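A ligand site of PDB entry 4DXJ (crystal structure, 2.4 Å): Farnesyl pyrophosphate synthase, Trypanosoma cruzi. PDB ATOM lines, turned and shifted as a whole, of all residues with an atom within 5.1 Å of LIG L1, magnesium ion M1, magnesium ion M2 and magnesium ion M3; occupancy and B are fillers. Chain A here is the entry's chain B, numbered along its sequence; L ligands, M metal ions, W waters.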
ATOM      1  N   TYR A  94     -30.813  25.748 -26.367  1.00  0.00           N
ATOM      2  CA  TYR A  94     -30.259  25.099 -25.196  1.00  0.00           C
ATOM      3  C   TYR A  94     -29.199  25.929 -24.478  1.00  0.00           C
ATOM      4  O   TYR A  94     -29.172  25.984 -23.256  1.00  0.00           O
ATOM      5  CB  TYR A  94     -29.819  23.638 -25.473  1.00  0.00           C
ATOM      6  CG  TYR A  94     -31.007  22.725 -25.303  1.00  0.00           C
ATOM      7  CD1 TYR A  94     -31.547  22.522 -24.035  1.00  0.00           C
ATOM      8  CD2 TYR A  94     -31.636  22.128 -26.387  1.00  0.00           C
ATOM      9  CE1 TYR A  94     -32.667  21.738 -23.838  1.00  0.00           C
ATOM     10  CE2 TYR A  94     -32.764  21.333 -26.204  1.00  0.00           C
ATOM     11  CZ  TYR A  94     -33.279  21.142 -24.919  1.00  0.00           C
ATOM     12  OH  TYR A  94     -34.398  20.372 -24.650  1.00  0.00           O
ATOM     13  N   LEU A  95     -28.361  26.622 -25.255  1.00  0.00           N
ATOM     14  CA  LEU A  95     -27.295  27.410 -24.661  1.00  0.00           C
ATOM     15  C   LEU A  95     -27.817  28.647 -23.937  1.00  0.00           C
ATOM     16  O   LEU A  95     -27.259  29.030 -22.893  1.00  0.00           O
ATOM     17  CB  LEU A  95     -26.203  27.761 -25.681  1.00  0.00           C
ATOM     18  CG  LEU A  95     -25.341  26.640 -26.267  1.00  0.00           C
ATOM     19  CD1 LEU A  95     -24.137  27.254 -26.988  1.00  0.00           C
ATOM     20  CD2 LEU A  95     -24.895  25.593 -25.235  1.00  0.00           C
ATOM     21  N   ASP A  98     -29.451  27.219 -20.814  1.00  0.00           N
ATOM     22  CA  ASP A  98     -28.391  26.615 -20.000  1.00  0.00           C
ATOM     23  C   ASP A  98     -27.512  27.650 -19.275  1.00  0.00           C
ATOM     24  O   ASP A  98     -27.152  27.450 -18.119  1.00  0.00           O
ATOM     25  CB  ASP A  98     -27.528  25.688 -20.838  1.00  0.00           C
ATOM     26  CG  ASP A  98     -26.357  25.141 -20.061  1.00  0.00           C
ATOM     27  OD1 ASP A  98     -26.511  24.109 -19.377  1.00  0.00           O
ATOM     28  OD2 ASP A  98     -25.252  25.741 -20.160  1.00  0.00           O
ATOM     29  N   ASP A  99     -27.184  28.736 -19.959  1.00  0.00           N
ATOM     30  CA  ASP A  99     -26.403  29.825 -19.349  1.00  0.00           C
ATOM     31  C   ASP A  99     -27.125  30.523 -18.212  1.00  0.00           C
ATOM     32  O   ASP A  99     -26.496  31.022 -17.285  1.00  0.00           O
ATOM     33  CB  ASP A  99     -25.966  30.844 -20.401  1.00  0.00           C
ATOM     34  CG  ASP A  99     -24.740  30.407 -21.133  1.00  0.00           C
ATOM     35  OD1 ASP A  99     -24.035  29.493 -20.628  1.00  0.00           O
ATOM     36  OD2 ASP A  99     -24.452  30.977 -22.205  1.00  0.00           O
ATOM     37  N   ASP A 102     -27.049  27.695 -15.350  1.00  0.00           N
ATOM     38  CA  ASP A 102     -25.722  27.504 -14.747  1.00  0.00           C
ATOM     39  C   ASP A 102     -25.094  28.775 -14.142  1.00  0.00           C
ATOM     40  O   ASP A 102     -24.027  28.720 -13.559  1.00  0.00           O
ATOM     41  CB  ASP A 102     -24.758  26.901 -15.773  1.00  0.00           C
ATOM     42  CG  ASP A 102     -25.251  25.578 -16.300  1.00  0.00           C
ATOM     43  OD1 ASP A 102     -26.114  24.983 -15.630  1.00  0.00           O
ATOM     44  OD2 ASP A 102     -24.785  25.139 -17.378  1.00  0.00           O
ATOM     45  N   SER A 104     -23.799  31.365 -15.776  1.00  0.00           N
ATOM     46  CA  SER A 104     -22.574  31.683 -16.523  1.00  0.00           C
ATOM     47  C   SER A 104     -22.494  33.139 -16.975  1.00  0.00           C
ATOM     48  O   SER A 104     -23.499  33.860 -16.993  1.00  0.00           O
ATOM     49  CB  SER A 104     -22.420  30.737 -17.721  1.00  0.00           C
ATOM     50  OG  SER A 104     -22.409  29.374 -17.311  1.00  0.00           O
ATOM     51  N   ARG A 107     -20.159  33.543 -23.260  1.00  0.00           N
ATOM     52  CA  ARG A 107     -20.466  32.507 -24.243  1.00  0.00           C
ATOM     53  C   ARG A 107     -19.890  32.935 -25.583  1.00  0.00           C
ATOM     54  O   ARG A 107     -20.266  33.972 -26.117  1.00  0.00           O
ATOM     55  CB  ARG A 107     -21.983  32.261 -24.324  1.00  0.00           C
ATOM     56  CG  ARG A 107     -22.463  31.259 -25.391  1.00  0.00           C
ATOM     57  CD  ARG A 107     -22.038  29.820 -25.122  1.00  0.00           C
ATOM     58  NE  ARG A 107     -22.695  29.227 -23.953  1.00  0.00           N
ATOM     59  CZ  ARG A 107     -22.524  27.971 -23.550  1.00  0.00           C
ATOM     60  NH1 ARG A 107     -21.729  27.139 -24.245  1.00  0.00           N
ATOM     61  NH2 ARG A 107     -23.157  27.537 -22.465  1.00  0.00           N
ATOM     62  N   THR A 163     -32.772  15.606 -24.567  1.00  0.00           N
ATOM     63  CA  THR A 163     -31.890  16.659 -24.082  1.00  0.00           C
ATOM     64  C   THR A 163     -32.466  17.347 -22.850  1.00  0.00           C
ATOM     65  O   THR A 163     -31.741  17.630 -21.888  1.00  0.00           O
ATOM     66  CB  THR A 163     -31.610  17.710 -25.184  1.00  0.00           C
ATOM     67  OG1 THR A 163     -31.264  17.036 -26.398  1.00  0.00           O
ATOM     68  CG2 THR A 163     -30.457  18.611 -24.783  1.00  0.00           C
ATOM     69  N   GLN A 167     -30.873  17.660 -19.329  1.00  0.00           N
ATOM     70  CA  GLN A 167     -30.696  18.903 -18.578  1.00  0.00           C
ATOM     71  C   GLN A 167     -31.267  18.782 -17.165  1.00  0.00           C
ATOM     72  O   GLN A 167     -30.723  19.364 -16.229  1.00  0.00           O
ATOM     73  CB  GLN A 167     -31.313  20.082 -19.329  1.00  0.00           C
ATOM     74  CG  GLN A 167     -30.466  20.596 -20.497  1.00  0.00           C
ATOM     75  CD  GLN A 167     -29.090  21.124 -20.076  1.00  0.00           C
ATOM     76  OE1 GLN A 167     -28.194  20.350 -19.732  1.00  0.00           O
ATOM     77  NE2 GLN A 167     -28.909  22.451 -20.131  1.00  0.00           N
ATOM     78  N   ASP A 170     -28.774  16.838 -15.240  1.00  0.00           N
ATOM     79  CA  ASP A 170     -27.593  17.653 -15.023  1.00  0.00           C
ATOM     80  C   ASP A 170     -27.809  18.637 -13.877  1.00  0.00           C
ATOM     81  O   ASP A 170     -26.978  18.768 -12.979  1.00  0.00           O
ATOM     82  CB  ASP A 170     -27.194  18.388 -16.301  1.00  0.00           C
ATOM     83  CG  ASP A 170     -26.070  19.377 -16.065  1.00  0.00           C
ATOM     84  OD1 ASP A 170     -24.891  18.971 -16.157  1.00  0.00           O
ATOM     85  OD2 ASP A 170     -26.368  20.571 -15.807  1.00  0.00           O
ATOM     86  N   LYS A 207     -28.064  14.703 -21.965  1.00  0.00           N
ATOM     87  CA  LYS A 207     -27.933  16.142 -22.180  1.00  0.00           C
ATOM     88  C   LYS A 207     -27.169  16.519 -23.444  1.00  0.00           C
ATOM     89  O   LYS A 207     -27.411  17.583 -24.003  1.00  0.00           O
ATOM     90  CB  LYS A 207     -27.346  16.857 -20.942  1.00  0.00           C
ATOM     91  CG  LYS A 207     -25.845  16.667 -20.728  1.00  0.00           C
ATOM     92  CD  LYS A 207     -25.323  17.679 -19.720  1.00  0.00           C
ATOM     93  CE  LYS A 207     -23.876  17.442 -19.383  1.00  0.00           C
ATOM     94  NZ  LYS A 207     -23.412  18.413 -18.366  1.00  0.00           N
ATOM     95  N   THR A 208     -26.283  15.642 -23.917  1.00  0.00           N
ATOM     96  CA  THR A 208     -25.356  16.013 -25.002  1.00  0.00           C
ATOM     97  C   THR A 208     -25.388  15.111 -26.229  1.00  0.00           C
ATOM     98  O   THR A 208     -25.435  15.585 -27.360  1.00  0.00           O
ATOM     99  CB  THR A 208     -23.901  16.090 -24.474  1.00  0.00           C
ATOM    100  OG1 THR A 208     -23.841  17.053 -23.422  1.00  0.00           O
ATOM    101  CG2 THR A 208     -22.916  16.502 -25.568  1.00  0.00           C
ATOM    102  N   TYR A 211     -28.303  15.257 -29.288  1.00  0.00           N
ATOM    103  CA  TYR A 211     -28.399  16.448 -30.127  1.00  0.00           C
ATOM    104  C   TYR A 211     -27.097  16.831 -30.788  1.00  0.00           C
ATOM    105  O   TYR A 211     -27.108  17.480 -31.841  1.00  0.00           O
ATOM    106  CB  TYR A 211     -29.044  17.623 -29.383  1.00  0.00           C
ATOM    107  CG  TYR A 211     -28.121  18.578 -28.648  1.00  0.00           C
ATOM    108  CD1 TYR A 211     -27.686  19.751 -29.250  1.00  0.00           C
ATOM    109  CD2 TYR A 211     -27.746  18.345 -27.333  1.00  0.00           C
ATOM    110  CE1 TYR A 211     -26.860  20.650 -28.570  1.00  0.00           C
ATOM    111  CE2 TYR A 211     -26.925  19.228 -26.651  1.00  0.00           C
ATOM    112  CZ  TYR A 211     -26.490  20.368 -27.269  1.00  0.00           C
ATOM    113  OH  TYR A 211     -25.678  21.229 -26.593  1.00  0.00           O
ATOM    114  N   GLN A 247     -18.302  15.595 -24.302  1.00  0.00           N
ATOM    115  CA  GLN A 247     -18.671  16.214 -23.045  1.00  0.00           C
ATOM    116  C   GLN A 247     -17.583  16.131 -21.980  1.00  0.00           C
ATOM    117  O   GLN A 247     -17.389  17.078 -21.212  1.00  0.00           O
ATOM    118  CB  GLN A 247     -19.968  15.631 -22.507  1.00  0.00           C
ATOM    119  CG  GLN A 247     -20.490  16.353 -21.262  1.00  0.00           C
ATOM    120  CD  GLN A 247     -20.887  17.780 -21.552  1.00  0.00           C
ATOM    121  OE1 GLN A 247     -21.699  18.033 -22.446  1.00  0.00           O
ATOM    122  NE2 GLN A 247     -20.344  18.731 -20.785  1.00  0.00           N
ATOM    123  N   ASP A 250     -15.291  18.910 -22.615  1.00  0.00           N
ATOM    124  CA  ASP A 250     -15.951  20.129 -22.149  1.00  0.00           C
ATOM    125  C   ASP A 250     -15.770  20.316 -20.644  1.00  0.00           C
ATOM    126  O   ASP A 250     -15.429  21.416 -20.190  1.00  0.00           O
ATOM    127  CB  ASP A 250     -17.441  20.071 -22.519  1.00  0.00           C
ATOM    128  CG  ASP A 250     -18.173  21.358 -22.180  1.00  0.00           C
ATOM    129  OD1 ASP A 250     -17.976  22.375 -22.887  1.00  0.00           O
ATOM    130  OD2 ASP A 250     -18.964  21.351 -21.208  1.00  0.00           O
ATOM    131  N   ASP A 251     -15.970  19.242 -19.874  1.00  0.00           N
ATOM    132  CA  ASP A 251     -15.760  19.296 -18.433  1.00  0.00           C
ATOM    133  C   ASP A 251     -14.308  19.633 -18.082  1.00  0.00           C
ATOM    134  O   ASP A 251     -14.048  20.428 -17.188  1.00  0.00           O
ATOM    135  CB  ASP A 251     -16.169  17.971 -17.765  1.00  0.00           C
ATOM    136  CG  ASP A 251     -17.652  17.673 -17.879  1.00  0.00           C
ATOM    137  OD1 ASP A 251     -18.419  18.480 -18.473  1.00  0.00           O
ATOM    138  OD2 ASP A 251     -18.054  16.606 -17.379  1.00  0.00           O
ATOM    139  N   ASP A 254     -13.558  23.271 -18.954  1.00  0.00           N
ATOM    140  CA  ASP A 254     -14.220  24.137 -17.983  1.00  0.00           C
ATOM    141  C   ASP A 254     -13.293  24.583 -16.859  1.00  0.00           C
ATOM    142  O   ASP A 254     -13.399  25.692 -16.347  1.00  0.00           O
ATOM    143  CB  ASP A 254     -15.403  23.414 -17.354  1.00  0.00           C
ATOM    144  CG  ASP A 254     -16.396  24.358 -16.764  1.00  0.00           C
ATOM    145  OD1 ASP A 254     -17.143  24.976 -17.552  1.00  0.00           O
ATOM    146  OD2 ASP A 254     -16.432  24.514 -15.532  1.00  0.00           O
ATOM    147  N   LYS A 264     -15.594  30.973 -23.039  1.00  0.00           N
ATOM    148  CA  LYS A 264     -16.549  30.920 -21.926  1.00  0.00           C
ATOM    149  C   LYS A 264     -15.824  30.779 -20.586  1.00  0.00           C
ATOM    150  O   LYS A 264     -14.668  30.390 -20.553  1.00  0.00           O
ATOM    151  CB  LYS A 264     -17.594  29.806 -22.134  1.00  0.00           C
ATOM    152  CG  LYS A 264     -17.033  28.431 -22.533  1.00  0.00           C
ATOM    153  CD  LYS A 264     -18.152  27.427 -22.787  1.00  0.00           C
ATOM    154  CE  LYS A 264     -17.618  26.007 -22.829  1.00  0.00           C
ATOM    155  NZ  LYS A 264     -18.664  25.017 -23.232  1.00  0.00           N
ATOM    156  N   ASP A 268     -18.487  24.922 -13.456  1.00  0.00           N
ATOM    157  CA  ASP A 268     -18.737  23.571 -12.939  1.00  0.00           C
ATOM    158  C   ASP A 268     -18.479  23.433 -11.441  1.00  0.00           C
ATOM    159  O   ASP A 268     -19.310  22.884 -10.713  1.00  0.00           O
ATOM    160  CB  ASP A 268     -17.928  22.534 -13.716  1.00  0.00           C
ATOM    161  CG  ASP A 268     -18.557  22.188 -15.043  1.00  0.00           C
ATOM    162  OD1 ASP A 268     -19.680  22.651 -15.334  1.00  0.00           O
ATOM    163  OD2 ASP A 268     -17.906  21.442 -15.810  1.00  0.00           O
ATOM    164  N   LYS A 273     -21.219  20.752 -10.079  1.00  0.00           N
ATOM    165  CA  LYS A 273     -21.631  19.822 -11.130  1.00  0.00           C
ATOM    166  C   LYS A 273     -20.978  18.458 -10.948  1.00  0.00           C
ATOM    167  O   LYS A 273     -19.853  18.349 -10.452  1.00  0.00           O
ATOM    168  CB  LYS A 273     -21.319  20.381 -12.527  1.00  0.00           C
ATOM    169  CG  LYS A 273     -22.225  21.572 -12.932  1.00  0.00           C
ATOM    170  CD  LYS A 273     -23.703  21.138 -12.997  1.00  0.00           C
ATOM    171  CE  LYS A 273     -24.642  22.303 -12.807  1.00  0.00           C
ATOM    172  NZ  LYS A 273     -24.707  23.204 -13.988  1.00  0.00           N
HETATM  173  O1  LIG L   1     -21.389  24.946 -22.828  1.00  0.00           O
HETATM  174  P1  LIG L   1     -21.576  24.666 -21.361  1.00  0.00           P
HETATM  175  O2  LIG L   1     -22.184  25.817 -20.618  1.00  0.00           O
HETATM  176  O3  LIG L   1     -20.350  24.095 -20.692  1.00  0.00           O
HETATM  177  C1  LIG L   1     -22.973  23.475 -21.228  1.00  0.00           C
HETATM  178  P2  LIG L   1     -22.858  22.371 -19.774  1.00  0.00           P
HETATM  179  O4  LIG L   1     -23.623  21.119 -20.082  1.00  0.00           O
HETATM  180  O5  LIG L   1     -23.629  23.252 -18.824  1.00  0.00           O
HETATM  181  O6  LIG L   1     -21.398  22.156 -19.476  1.00  0.00           O
HETATM  182  C2  LIG L   1     -23.236  22.637 -22.477  1.00  0.00           C
HETATM  183  N1  LIG L   1     -24.668  22.488 -22.543  1.00  0.00           N
HETATM  184  C3  LIG L   1     -25.267  21.373 -23.246  1.00  0.00           C
HETATM  185  C4  LIG L   1     -26.578  20.968 -22.590  1.00  0.00           C
HETATM  186  C5  LIG L   1     -27.709  20.858 -23.591  1.00  0.00           C
HETATM  187  C1  LG2 L   2     -22.052  22.293 -27.101  1.00  0.00           C
HETATM  188  O1  LG2 L   2     -21.230  23.447 -27.137  1.00  0.00           O
HETATM  189  C2  LG2 L   2     -22.518  22.104 -25.665  1.00  0.00           C
HETATM  190  C3  LG2 L   2     -21.318  21.777 -24.813  1.00  0.00           C
HETATM  191  C4  LG2 L   2     -20.473  22.740 -24.460  1.00  0.00           C
HETATM  192  C5  LG2 L   2     -21.074  20.368 -24.370  1.00  0.00           C
HETATM  193  P1  LG2 L   2     -20.129  23.663 -28.292  1.00  0.00           P
HETATM  194  O2  LG2 L   2     -18.755  23.535 -27.654  1.00  0.00           O
HETATM  195  O3  LG2 L   2     -20.493  22.849 -29.517  1.00  0.00           O
HETATM  196  O4  LG2 L   2     -20.384  25.242 -28.572  1.00  0.00           O
HETATM  197  P2  LG2 L   2     -20.382  25.967 -30.013  1.00  0.00           P
HETATM  198  O5  LG2 L   2     -19.935  27.347 -29.590  1.00  0.00           O
HETATM  199  O6  LG2 L   2     -19.420  25.205 -30.898  1.00  0.00           O
HETATM  200  O7  LG2 L   2     -21.826  25.869 -30.446  1.00  0.00           O
HETATM  201 MG    MG M   1     -25.389  22.973 -18.105  1.00  0.00          MG
HETATM  202 MG    MG M   2     -23.378  25.280 -19.045  1.00  0.00          MG
HETATM  203 MG    MG M   3     -19.390  22.725 -19.714  1.00  0.00          MG
HETATM  204  O   HOH W   1     -22.190  25.489 -17.681  1.00  0.00           O
HETATM  205  O   HOH W   2     -27.050  22.974 -16.841  1.00  0.00           O
HETATM  206  O   HOH W   3     -19.559  23.974 -18.025  1.00  0.00           O
HETATM  207  O   HOH W   4     -21.755  21.419 -16.702  1.00  0.00           O
HETATM  208  O   HOH W   5     -24.286  22.039 -16.537  1.00  0.00           O
HETATM  209  O   HOH W   6     -18.909  21.264 -18.386  1.00  0.00           O
HETATM  210  O   HOH W   7     -20.222  27.388 -19.874  1.00  0.00           O
HETATM  211  O   HOH W   8     -25.962  21.208 -18.667  1.00  0.00           O
HETATM  212  O   HOH W   9     -17.478  23.326 -20.092  1.00  0.00           O
HETATM  213  O   HOH W  10     -23.534  27.457 -18.909  1.00  0.00           O
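O1 of LIG L1 lies within salt-bridge range of NH1 of Arg 107.
An oxygen (O1) of LIG L1 lies within salt-bridge range of the side-chain amino group (NZ) of Lys 264.
An oxygen (O4) of LIG L1 is in salt-bridge range of the side-chain amino group (NZ) of Lys 207, 3.2 Å away.
Water W5 lies within hydrogen-bond range of OD2 of Asp 170 (2.7 Å) and NZ of Lys 273 (2.8 Å).
Water W2 bridges the side-chain carboxylate (OD1) of Asp 102 (2.5 Å) and the side-chain carboxylate (OD2) of Asp 170 (2.7 Å).
Water W10 bridges OD1 of Asp 99 (2.7 Å) and OG of Ser 104 (2.7 Å).
Water W9 lies within hydrogen-bond range of the backbone carbonyl oxygen of Asp 250 (2.8 Å) and the side-chain carboxylate of Asp 254 (3.0 Å).
Water W6 bridges OD2 of Asp 268 (2.8 Å) and OD1 of Asp 251 (2.8 Å).
Water W3 lies within hydrogen-bond range of OD1 of Asp 254 (2.7 Å) and OD1 of Asp 268 (3.0 Å).
NZ of Lys 264 is in salt-bridge range of OD1 of Asp 250, at 2.8 Å.
OD2 of Asp 250 lies close to NE2 of Gln 247, 3.0 Å away.
OD1 of Asp 102 is in salt-bridge range of NZ of Lys 273 (2.8 Å).
The guanidinium group of Arg 107 lies within salt-bridge range of the side-chain carboxylate of Asp 99 (2.8 Å).
OD1 of Asp 170 is in salt-bridge range of NZ of Lys 207 (2.7 Å).
The side-chain carboxylate (OD1) of Asp 251 is in hydrogen-bond range of the side-chain amide nitrogen (NE2) of Gln 247 (3.0 Å).
The side-chain hydroxyl (OG1) of Thr 208 sits at hydrogen-bond distance from the side-chain amide oxygen (OE1) of Gln 247, 2.5 Å away.
N of Asp 268 is in hydrogen-bond range of OD2 of Asp 254 (2.9 Å).
Tyr 94 touches LIG L1 (CB to C5, 3.97 Å).
Thr 163 touches LIG L1 (CG2 to C5, 3.7 Å).
OE1 of Gln 167 touches C4 of LIG L1 (3.3 Å).
OH of Tyr 211 touches C3 of LIG L1, 3.4 Å away.
NE2 of Gln 247 touches O6 of LIG L1 (3.8 Å).
Within 4 Å of LIG L1: Tyr 94, Asp 98, Asp 102, Arg 107, Thr 163, Gln 167, Lys 207, Tyr 211, Gln 247, Asp 250 and Lys 264.
Along chain A the residues within 4 Å of LIG L1 span positions 94 to 264.
The nearest printed residue that does not touch LIG L1 is Asp 99 (4.1 Å).
Merely in contact with magnesium ion M3: Asp 254 (3.8 Å).
Within 4 Å of magnesium ion M3: Asp 250 and Asp 254.
The nearest printed residue that does not touch magnesium ion M3 is Gln 247 (4.2 Å).
O5 of LIG L1 is bound to magnesium ion M1, 1.9 Å away.
Magnesium ion M1 is bound by water W8 (1.9 Å).
OD1 of Asp 98 binds magnesium ion M1.
Water W2 binds magnesium ion M1 (2.1 Å).
Magnesium ion M1 is bound by water W5 (2.1 Å).
Magnesium ion M1 is bound by the side-chain carboxylate (OD2) of Asp 102 (2.4 Å).
Magnesium ion M2 is bound by water W1, at 1.8 Å.
Magnesium ion M2 is bound by an oxygen (O2) of LIG L1, at 2.0 Å.
Magnesium ion M2 is bound by O5 of LIG L1, at 2.1 Å.
OD2 of Asp 102 binds magnesium ion M2 (2.2 Å).
Water W10 binds magnesium ion M2 (2.2 Å).
The side-chain carboxylate (OD2) of Asp 98 is bound to magnesium ion M2, at 2.2 Å.
Two residues have an atom within 4 Å of magnesium ion M2: Asp 98 and Asp 102.
The nearest printed residue that does not touch magnesium ion M2 is Arg 107 (4.1 Å).
Merely in contact with magnesium ion M1: Asp 170.
The nearest printed residue that does not touch magnesium ion M1 is Gln 167 (4.1 Å).
Magnesium ion M3 is bound by O3 of LIG L1 (1.9 Å), water W6 (2.0 Å), water W9 (2.0 Å), OD2 of Asp 250 (2.1 Å), O6 of LIG L1 (2.1 Å) and water W3 (2.1 Å).
Magnesium ion M3 has six donor atoms within binding distance.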
